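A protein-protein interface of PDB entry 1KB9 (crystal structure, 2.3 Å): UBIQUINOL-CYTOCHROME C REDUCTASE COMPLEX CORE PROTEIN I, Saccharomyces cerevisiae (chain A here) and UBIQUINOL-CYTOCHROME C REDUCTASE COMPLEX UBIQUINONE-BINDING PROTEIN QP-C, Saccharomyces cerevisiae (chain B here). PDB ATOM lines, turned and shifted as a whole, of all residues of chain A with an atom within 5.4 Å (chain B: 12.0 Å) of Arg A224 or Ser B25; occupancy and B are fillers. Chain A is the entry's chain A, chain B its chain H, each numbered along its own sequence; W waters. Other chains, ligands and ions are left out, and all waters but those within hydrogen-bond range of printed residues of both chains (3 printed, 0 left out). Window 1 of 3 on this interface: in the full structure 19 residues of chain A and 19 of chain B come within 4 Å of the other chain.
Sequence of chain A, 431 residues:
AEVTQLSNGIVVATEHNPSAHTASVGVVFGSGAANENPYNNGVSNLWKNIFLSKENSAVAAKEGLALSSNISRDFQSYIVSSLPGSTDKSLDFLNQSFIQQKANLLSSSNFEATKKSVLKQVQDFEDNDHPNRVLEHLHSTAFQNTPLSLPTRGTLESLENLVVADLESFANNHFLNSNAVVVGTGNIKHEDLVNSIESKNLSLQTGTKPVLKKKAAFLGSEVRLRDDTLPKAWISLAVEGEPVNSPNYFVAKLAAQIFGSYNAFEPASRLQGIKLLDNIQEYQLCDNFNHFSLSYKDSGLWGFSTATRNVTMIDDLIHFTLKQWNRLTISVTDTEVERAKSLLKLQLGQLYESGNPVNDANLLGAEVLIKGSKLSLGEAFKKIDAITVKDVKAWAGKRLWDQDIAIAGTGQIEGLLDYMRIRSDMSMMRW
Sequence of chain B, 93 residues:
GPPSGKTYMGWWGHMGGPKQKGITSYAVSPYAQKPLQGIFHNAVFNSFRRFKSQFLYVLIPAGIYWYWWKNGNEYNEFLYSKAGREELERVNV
The guanidinium group (NH2) of Arg A224 lies within salt-bridge range of the side-chain carboxylate (OE2) of Glu A222, 2.8 Å away.
O of Ile A407 lies within hydrogen-bond range of N of Val A223 (3.0 Å).
O of Val A223 sits at hydrogen-bond distance from N of Gly A409 (3.3 Å).
The guanidinium group (NH1) of Arg A224 lies within hydrogen-bond range of the backbone carbonyl oxygen (O) of Leu A416, at 2.5 Å.
O of Leu A417 lies within hydrogen-bond range of NH1 of Arg A224 (2.8 Å).
The backbone carbonyl oxygen of Gly A409 is in hydrogen-bond range of the backbone NH of Leu A225 (2.8 Å).
Arg A224 touches just these residues of chain B: Ile B23 (3.97 Å), Thr B24 (3.3 Å) and Ser B25 (2.9 Å).
Of the printed residues of chain A, Ser B25 touches Val A223 and Arg A224.
Glu A222 touches two residues of chain B.
Of chain B, only Thr B24 (3.8 Å), Ser B25 (3.4 Å) and Tyr B26 (3.6 Å) come within 4 Å of Val A223.
No residue of chain B comes within 4 Å of Gly A409.
No residue of chain B comes within 4 Å of Leu A416.
No residue of chain B comes within 4 Å of Asp A418.
Printed residues of chain A within 4 Å of Ala B27: Glu A222 (3.0 Å).
Of the printed residues of chain B, Tyr A419 touches Ser B29.
Lys B21 touches none of the printed residues of chain A.
Pro B30 touches none of the printed residues of chain A.
The nearest residue of chain B that does not touch Arg A224 is Tyr B26 (5.1 Å).
The nearest printed residue of chain A that does not touch Ser B29 is Glu A222 (6.0 Å).
The backbone NH (N) of Glu A222 lies within hydrogen-bond range of the backbone carbonyl oxygen (O) of Ala B27 (3.0 Å).
The backbone carbonyl oxygen (O) of Ser B25 is in hydrogen-bond range of the backbone NH (N) of Arg A224.
The side-chain amide oxygen (OE1) of Gln B20 is in hydrogen-bond range of the guanidinium group (NE) of Arg A226.
Hydrophobic or aromatic side chains of chain A that line the printed part of chain B: Val A223, Leu A225 and Tyr A419.
Hydrophobic or aromatic side chains of chain B within 4 Å of the printed part of chain A: Tyr B26 and Ala B27.
Among the printed residues, 12 pairs touch across the chains.
Among the printed residues, no Asp or Glu carboxylate lies within 4 Å of a Lys or Arg side-chain nitrogen of the other chain.
Water W3 lies within hydrogen-bond range of O of Arg A226 (2.7 Å), O of Ile B23 (3.0 Å), N of Lys B21 (3.3 Å) and N of Gly B22 (3.5 Å).
Water W1 lies within hydrogen-bond range of OG1 of Thr B24, O of Ile B23 and O of Arg A226.
Water W2 bridges O of Glu A222 (3.2 Å) and O of Ala B27 (3.3 Å).
Glu A222 touches Tyr B26.
Val A223 touches Thr B24 (CG2 to CG2, 3.8 Å).
CA of Val A223 touches O of Ser B25 (3.4 Å).
CG2 of Val A223 touches CE2 of Tyr B26, at 3.6 Å.
O of Arg A224 touches O of Ile B23, 3.97 Å away.
O of Arg A224 touches CA of Thr B24, at 3.3 Å.
CD2 of Leu A225 touches OG1 of Thr B24 (3.7 Å).
Arg A226 touches Ile B23.
Tyr A419 touches Ser B29 (CE2 to CB, 3.4 Å).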
ATOM      1  N   GLU A 222       3.278 -18.293  24.831  1.00  0.00           N
ATOM      2  CA  GLU A 222       2.715 -19.005  23.689  1.00  0.00           C
ATOM      3  C   GLU A 222       2.584 -18.128  22.456  1.00  0.00           C
ATOM      4  O   GLU A 222       2.571 -16.906  22.555  1.00  0.00           O
ATOM      5  CB  GLU A 222       1.319 -19.521  24.048  1.00  0.00           C
ATOM      6  CG  GLU A 222       0.322 -18.401  24.405  1.00  0.00           C
ATOM      7  CD  GLU A 222      -1.078 -18.904  24.722  1.00  0.00           C
ATOM      8  OE1 GLU A 222      -2.037 -18.120  24.590  1.00  0.00           O
ATOM      9  OE2 GLU A 222      -1.225 -20.079  25.104  1.00  0.00           O
ATOM     10  N   VAL A 223       2.517 -18.771  21.294  1.00  0.00           N
ATOM     11  CA  VAL A 223       2.315 -18.090  20.021  1.00  0.00           C
ATOM     12  C   VAL A 223       1.326 -18.977  19.273  1.00  0.00           C
ATOM     13  O   VAL A 223       1.556 -20.165  19.097  1.00  0.00           O
ATOM     14  CB  VAL A 223       3.633 -17.875  19.204  1.00  0.00           C
ATOM     15  CG1 VAL A 223       4.411 -19.175  19.029  1.00  0.00           C
ATOM     16  CG2 VAL A 223       3.306 -17.265  17.840  1.00  0.00           C
ATOM     17  N   ARG A 224       0.180 -18.420  18.911  1.00  0.00           N
ATOM     18  CA  ARG A 224      -0.841 -19.201  18.229  1.00  0.00           C
ATOM     19  C   ARG A 224      -1.009 -18.711  16.801  1.00  0.00           C
ATOM     20  O   ARG A 224      -1.398 -17.572  16.564  1.00  0.00           O
ATOM     21  CB  ARG A 224      -2.147 -19.169  19.051  1.00  0.00           C
ATOM     22  CG  ARG A 224      -1.917 -19.685  20.488  1.00  0.00           C
ATOM     23  CD  ARG A 224      -3.026 -19.360  21.499  1.00  0.00           C
ATOM     24  NE  ARG A 224      -3.966 -20.467  21.611  1.00  0.00           N
ATOM     25  CZ  ARG A 224      -4.148 -21.220  22.693  1.00  0.00           C
ATOM     26  NH1 ARG A 224      -5.020 -22.203  22.637  1.00  0.00           N
ATOM     27  NH2 ARG A 224      -3.502 -20.989  23.828  1.00  0.00           N
ATOM     28  N   LEU A 225      -0.618 -19.559  15.854  1.00  0.00           N
ATOM     29  CA  LEU A 225      -0.680 -19.241  14.426  1.00  0.00           C
ATOM     30  C   LEU A 225      -1.913 -19.882  13.791  1.00  0.00           C
ATOM     31  O   LEU A 225      -1.799 -20.648  12.836  1.00  0.00           O
ATOM     32  CB  LEU A 225       0.603 -19.746  13.739  1.00  0.00           C
ATOM     33  CG  LEU A 225       1.930 -19.250  14.340  1.00  0.00           C
ATOM     34  CD1 LEU A 225       2.945 -20.365  14.395  1.00  0.00           C
ATOM     35  CD2 LEU A 225       2.478 -18.065  13.547  1.00  0.00           C
ATOM     36  N   ARG A 226      -3.094 -19.536  14.293  1.00  0.00           N
ATOM     37  CA  ARG A 226      -4.324 -20.125  13.776  1.00  0.00           C
ATOM     38  C   ARG A 226      -4.484 -19.972  12.280  1.00  0.00           C
ATOM     39  O   ARG A 226      -4.216 -18.914  11.727  1.00  0.00           O
ATOM     40  CB  ARG A 226      -5.574 -19.571  14.474  1.00  0.00           C
ATOM     41  CG  ARG A 226      -6.679 -20.624  14.539  1.00  0.00           C
ATOM     42  CD  ARG A 226      -8.070 -20.109  14.245  1.00  0.00           C
ATOM     43  NE  ARG A 226      -8.841 -19.889  15.457  1.00  0.00           N
ATOM     44  CZ  ARG A 226     -10.160 -20.031  15.563  1.00  0.00           C
ATOM     45  NH1 ARG A 226     -10.736 -19.793  16.729  1.00  0.00           N
ATOM     46  NH2 ARG A 226     -10.903 -20.423  14.536  1.00  0.00           N
ATOM     47  N   ILE A 407       4.102 -22.770  24.452  1.00  0.00           N
ATOM     48  CA  ILE A 407       3.225 -23.401  23.465  1.00  0.00           C
ATOM     49  C   ILE A 407       3.289 -22.699  22.112  1.00  0.00           C
ATOM     50  O   ILE A 407       3.430 -21.486  22.046  1.00  0.00           O
ATOM     51  CB  ILE A 407       1.728 -23.359  23.949  1.00  0.00           C
ATOM     52  CG1 ILE A 407       1.599 -23.946  25.352  1.00  0.00           C
ATOM     53  CG2 ILE A 407       0.814 -24.118  22.990  1.00  0.00           C
ATOM     54  CD1 ILE A 407       0.216 -23.830  25.916  1.00  0.00           C
ATOM     55  N   GLY A 409       1.474 -23.298  17.945  1.00  0.00           N
ATOM     56  CA  GLY A 409       0.627 -24.137  17.117  1.00  0.00           C
ATOM     57  C   GLY A 409       0.118 -23.449  15.869  1.00  0.00           C
ATOM     58  O   GLY A 409       0.125 -22.228  15.782  1.00  0.00           O
ATOM     59  N   ILE A 413      -6.502 -24.781  15.362  1.00  0.00           N
ATOM     60  CA  ILE A 413      -6.277 -24.825  16.804  1.00  0.00           C
ATOM     61  C   ILE A 413      -7.319 -24.094  17.672  1.00  0.00           C
ATOM     62  O   ILE A 413      -7.011 -23.648  18.783  1.00  0.00           O
ATOM     63  CB  ILE A 413      -4.859 -24.325  17.172  1.00  0.00           C
ATOM     64  CG1 ILE A 413      -4.602 -22.944  16.567  1.00  0.00           C
ATOM     65  CG2 ILE A 413      -3.812 -25.309  16.677  1.00  0.00           C
ATOM     66  CD1 ILE A 413      -3.302 -22.310  17.025  1.00  0.00           C
ATOM     67  N   LEU A 416      -7.693 -25.788  20.975  1.00  0.00           N
ATOM     68  CA  LEU A 416      -6.580 -25.781  21.917  1.00  0.00           C
ATOM     69  C   LEU A 416      -6.983 -24.731  22.932  1.00  0.00           C
ATOM     70  O   LEU A 416      -7.158 -23.570  22.589  1.00  0.00           O
ATOM     71  CB  LEU A 416      -5.268 -25.394  21.213  1.00  0.00           C
ATOM     72  CG  LEU A 416      -3.999 -25.291  22.074  1.00  0.00           C
ATOM     73  CD1 LEU A 416      -3.572 -26.669  22.546  1.00  0.00           C
ATOM     74  CD2 LEU A 416      -2.872 -24.628  21.297  1.00  0.00           C
ATOM     75  N   LEU A 417      -7.219 -25.152  24.163  1.00  0.00           N
ATOM     76  CA  LEU A 417      -7.652 -24.226  25.203  1.00  0.00           C
ATOM     77  C   LEU A 417      -6.623 -23.168  25.597  1.00  0.00           C
ATOM     78  O   LEU A 417      -5.470 -23.219  25.180  1.00  0.00           O
ATOM     79  CB  LEU A 417      -8.123 -25.013  26.428  1.00  0.00           C
ATOM     80  CG  LEU A 417      -9.620 -25.363  26.504  1.00  0.00           C
ATOM     81  CD1 LEU A 417     -10.229 -25.544  25.129  1.00  0.00           C
ATOM     82  CD2 LEU A 417      -9.835 -26.587  27.378  1.00  0.00           C
ATOM     83  N   ASP A 418      -7.065 -22.203  26.391  1.00  0.00           N
ATOM     84  CA  ASP A 418      -6.225 -21.113  26.873  1.00  0.00           C
ATOM     85  C   ASP A 418      -4.993 -21.596  27.636  1.00  0.00           C
ATOM     86  O   ASP A 418      -4.953 -22.711  28.146  1.00  0.00           O
ATOM     87  CB  ASP A 418      -7.036 -20.225  27.801  1.00  0.00           C
ATOM     88  CG  ASP A 418      -7.607 -21.001  28.950  1.00  0.00           C
ATOM     89  OD1 ASP A 418      -8.523 -21.804  28.694  1.00  0.00           O
ATOM     90  OD2 ASP A 418      -7.102 -20.866  30.087  1.00  0.00           O
ATOM     91  N   TYR A 419      -4.032 -20.693  27.785  1.00  0.00           N
ATOM     92  CA  TYR A 419      -2.791 -20.988  28.471  1.00  0.00           C
ATOM     93  C   TYR A 419      -2.984 -21.557  29.865  1.00  0.00           C
ATOM     94  O   TYR A 419      -2.487 -22.646  30.153  1.00  0.00           O
ATOM     95  CB  TYR A 419      -1.908 -19.739  28.533  1.00  0.00           C
ATOM     96  CG  TYR A 419      -0.522 -20.016  29.074  1.00  0.00           C
ATOM     97  CD1 TYR A 419       0.503 -20.455  28.228  1.00  0.00           C
ATOM     98  CD2 TYR A 419      -0.238 -19.856  30.437  1.00  0.00           C
ATOM     99  CE1 TYR A 419       1.777 -20.726  28.721  1.00  0.00           C
ATOM    100  CE2 TYR A 419       1.027 -20.129  30.943  1.00  0.00           C
ATOM    101  CZ  TYR A 419       2.033 -20.565  30.077  1.00  0.00           C
ATOM    102  OH  TYR A 419       3.288 -20.847  30.570  1.00  0.00           O
ATOM    103  N   TRP B  12     -16.022 -25.963  21.012  1.00  0.00           N
ATOM    104  CA  TRP B  12     -14.592 -25.951  20.707  1.00  0.00           C
ATOM    105  C   TRP B  12     -14.250 -26.789  19.478  1.00  0.00           C
ATOM    106  O   TRP B  12     -14.514 -28.000  19.445  1.00  0.00           O
ATOM    107  CB  TRP B  12     -13.807 -26.447  21.913  1.00  0.00           C
ATOM    108  CG  TRP B  12     -14.058 -25.622  23.127  1.00  0.00           C
ATOM    109  CD1 TRP B  12     -14.759 -25.988  24.229  1.00  0.00           C
ATOM    110  CD2 TRP B  12     -13.605 -24.283  23.362  1.00  0.00           C
ATOM    111  NE1 TRP B  12     -14.775 -24.965  25.143  1.00  0.00           N
ATOM    112  CE2 TRP B  12     -14.070 -23.905  24.637  1.00  0.00           C
ATOM    113  CE3 TRP B  12     -12.848 -23.366  22.616  1.00  0.00           C
ATOM    114  CZ2 TRP B  12     -13.799 -22.643  25.197  1.00  0.00           C
ATOM    115  CZ3 TRP B  12     -12.576 -22.111  23.171  1.00  0.00           C
ATOM    116  CH2 TRP B  12     -13.049 -21.764  24.449  1.00  0.00           C
ATOM    117  N   GLY B  13     -13.705 -26.132  18.454  1.00  0.00           N
ATOM    118  CA  GLY B  13     -13.361 -26.830  17.229  1.00  0.00           C
ATOM    119  C   GLY B  13     -14.361 -26.570  16.111  1.00  0.00           C
ATOM    120  O   GLY B  13     -14.049 -26.792  14.937  1.00  0.00           O
ATOM    121  N   MET B  15     -16.974 -23.649  16.517  1.00  0.00           N
ATOM    122  CA  MET B  15     -17.727 -22.574  17.153  1.00  0.00           C
ATOM    123  C   MET B  15     -18.776 -21.931  16.270  1.00  0.00           C
ATOM    124  O   MET B  15     -19.760 -21.382  16.774  1.00  0.00           O
ATOM    125  CB  MET B  15     -16.786 -21.501  17.696  1.00  0.00           C
ATOM    126  CG  MET B  15     -17.317 -20.798  18.935  1.00  0.00           C
ATOM    127  SD  MET B  15     -17.500 -21.930  20.331  1.00  0.00           S
ATOM    128  CE  MET B  15     -15.792 -22.106  20.849  1.00  0.00           C
ATOM    129  N   GLN B  20     -10.622 -18.401  10.143  1.00  0.00           N
ATOM    130  CA  GLN B  20      -9.589 -17.429  10.482  1.00  0.00           C
ATOM    131  C   GLN B  20      -8.254 -17.786   9.855  1.00  0.00           C
ATOM    132  O   GLN B  20      -7.851 -18.946   9.852  1.00  0.00           O
ATOM    133  CB  GLN B  20      -9.427 -17.326  12.003  1.00  0.00           C
ATOM    134  CG  GLN B  20     -10.662 -16.838  12.738  1.00  0.00           C
ATOM    135  CD  GLN B  20     -10.438 -16.740  14.234  1.00  0.00           C
ATOM    136  OE1 GLN B  20      -9.308 -16.571  14.688  1.00  0.00           O
ATOM    137  NE2 GLN B  20     -11.513 -16.850  15.009  1.00  0.00           N
ATOM    138  N   LYS B  21      -7.559 -16.774   9.347  1.00  0.00           N
ATOM    139  CA  LYS B  21      -6.258 -16.956   8.713  1.00  0.00           C
ATOM    140  C   LYS B  21      -5.520 -15.621   8.764  1.00  0.00           C
ATOM    141  O   LYS B  21      -6.133 -14.570   8.589  1.00  0.00           O
ATOM    142  CB  LYS B  21      -6.447 -17.386   7.258  1.00  0.00           C
ATOM    143  CG  LYS B  21      -5.181 -17.862   6.556  1.00  0.00           C
ATOM    144  CD  LYS B  21      -5.472 -18.181   5.082  1.00  0.00           C
ATOM    145  CE  LYS B  21      -4.425 -19.107   4.464  1.00  0.00           C
ATOM    146  NZ  LYS B  21      -3.049 -18.571   4.588  1.00  0.00           N
ATOM    147  N   GLY B  22      -4.222 -15.661   9.050  1.00  0.00           N
ATOM    148  CA  GLY B  22      -3.435 -14.443   9.101  1.00  0.00           C
ATOM    149  C   GLY B  22      -3.285 -13.776  10.453  1.00  0.00           C
ATOM    150  O   GLY B  22      -2.433 -12.900  10.625  1.00  0.00           O
ATOM    151  N   ILE B  23      -4.127 -14.157  11.408  1.00  0.00           N
ATOM    152  CA  ILE B  23      -4.075 -13.584  12.753  1.00  0.00           C
ATOM    153  C   ILE B  23      -3.198 -14.468  13.636  1.00  0.00           C
ATOM    154  O   ILE B  23      -3.404 -15.677  13.712  1.00  0.00           O
ATOM    155  CB  ILE B  23      -5.485 -13.506  13.371  1.00  0.00           C
ATOM    156  CG1 ILE B  23      -6.428 -12.754  12.427  1.00  0.00           C
ATOM    157  CG2 ILE B  23      -5.423 -12.849  14.749  1.00  0.00           C
ATOM    158  CD1 ILE B  23      -7.894 -12.913  12.752  1.00  0.00           C
ATOM    159  N   THR B  24      -2.226 -13.856  14.301  1.00  0.00           N
ATOM    160  CA  THR B  24      -1.312 -14.564  15.183  1.00  0.00           C
ATOM    161  C   THR B  24      -1.408 -13.919  16.562  1.00  0.00           C
ATOM    162  O   THR B  24      -1.332 -12.698  16.680  1.00  0.00           O
ATOM    163  CB  THR B  24       0.151 -14.456  14.645  1.00  0.00           C
ATOM    164  OG1 THR B  24       0.236 -15.108  13.375  1.00  0.00           O
ATOM    165  CG2 THR B  24       1.155 -15.093  15.599  1.00  0.00           C
ATOM    166  N   SER B  25      -1.591 -14.724  17.607  1.00  0.00           N
ATOM    167  CA  SER B  25      -1.694 -14.163  18.950  1.00  0.00           C
ATOM    168  C   SER B  25      -0.528 -14.564  19.824  1.00  0.00           C
ATOM    169  O   SER B  25       0.086 -15.606  19.618  1.00  0.00           O
ATOM    170  CB  SER B  25      -3.023 -14.551  19.619  1.00  0.00           C
ATOM    171  OG  SER B  25      -3.118 -15.948  19.846  1.00  0.00           O
ATOM    172  N   TYR B  26      -0.224 -13.725  20.802  1.00  0.00           N
ATOM    173  CA  TYR B  26       0.881 -13.990  21.711  1.00  0.00           C
ATOM    174  C   TYR B  26       0.417 -13.719  23.125  1.00  0.00           C
ATOM    175  O   TYR B  26      -0.382 -12.809  23.352  1.00  0.00           O
ATOM    176  CB  TYR B  26       2.063 -13.057  21.417  1.00  0.00           C
ATOM    177  CG  TYR B  26       2.612 -13.126  20.010  1.00  0.00           C
ATOM    178  CD1 TYR B  26       1.996 -12.432  18.967  1.00  0.00           C
ATOM    179  CD2 TYR B  26       3.781 -13.838  19.729  1.00  0.00           C
ATOM    180  CE1 TYR B  26       2.531 -12.443  17.686  1.00  0.00           C
ATOM    181  CE2 TYR B  26       4.328 -13.849  18.448  1.00  0.00           C
ATOM    182  CZ  TYR B  26       3.701 -13.150  17.434  1.00  0.00           C
ATOM    183  OH  TYR B  26       4.246 -13.139  16.169  1.00  0.00           O
ATOM    184  N   ALA B  27       0.946 -14.478  24.077  1.00  0.00           N
ATOM    185  CA  ALA B  27       0.596 -14.287  25.473  1.00  0.00           C
ATOM    186  C   ALA B  27       1.754 -14.753  26.353  1.00  0.00           C
ATOM    187  O   ALA B  27       2.597 -15.535  25.920  1.00  0.00           O
ATOM    188  CB  ALA B  27      -0.699 -15.048  25.820  1.00  0.00           C
ATOM    189  N   VAL B  28       1.758 -14.294  27.598  1.00  0.00           N
ATOM    190  CA  VAL B  28       2.804 -14.635  28.542  1.00  0.00           C
ATOM    191  C   VAL B  28       2.190 -15.097  29.860  1.00  0.00           C
ATOM    192  O   VAL B  28       1.269 -14.466  30.385  1.00  0.00           O
ATOM    193  CB  VAL B  28       3.729 -13.409  28.796  1.00  0.00           C
ATOM    194  CG1 VAL B  28       4.672 -13.679  29.956  1.00  0.00           C
ATOM    195  CG2 VAL B  28       4.537 -13.098  27.541  1.00  0.00           C
ATOM    196  N   SER B  29       2.727 -16.187  30.399  1.00  0.00           N
ATOM    197  CA  SER B  29       2.247 -16.752  31.646  1.00  0.00           C
ATOM    198  C   SER B  29       2.093 -15.730  32.760  1.00  0.00           C
ATOM    199  O   SER B  29       2.936 -14.845  32.929  1.00  0.00           O
ATOM    200  CB  SER B  29       3.190 -17.854  32.129  1.00  0.00           C
ATOM    201  OG  SER B  29       2.838 -18.295  33.434  1.00  0.00           O
ATOM    202  N   PRO B  30       0.971 -15.804  33.497  1.00  0.00           N
ATOM    203  CA  PRO B  30       0.694 -14.898  34.612  1.00  0.00           C
ATOM    204  C   PRO B  30       1.778 -15.079  35.669  1.00  0.00           C
ATOM    205  O   PRO B  30       2.045 -14.177  36.457  1.00  0.00           O
ATOM    206  CB  PRO B  30      -0.651 -15.405  35.125  1.00  0.00           C
ATOM    207  CG  PRO B  30      -1.329 -15.839  33.862  1.00  0.00           C
ATOM    208  CD  PRO B  30      -0.227 -16.596  33.156  1.00  0.00           C
HETATM  209  O   HOH W   1      -1.268 -17.142  11.688  1.00  0.00           O
HETATM  210  O   HOH W   2       4.632 -14.638  23.529  1.00  0.00           O
HETATM  211  O   HOH W   3      -5.695 -16.677  12.055  1.00  0.00           O
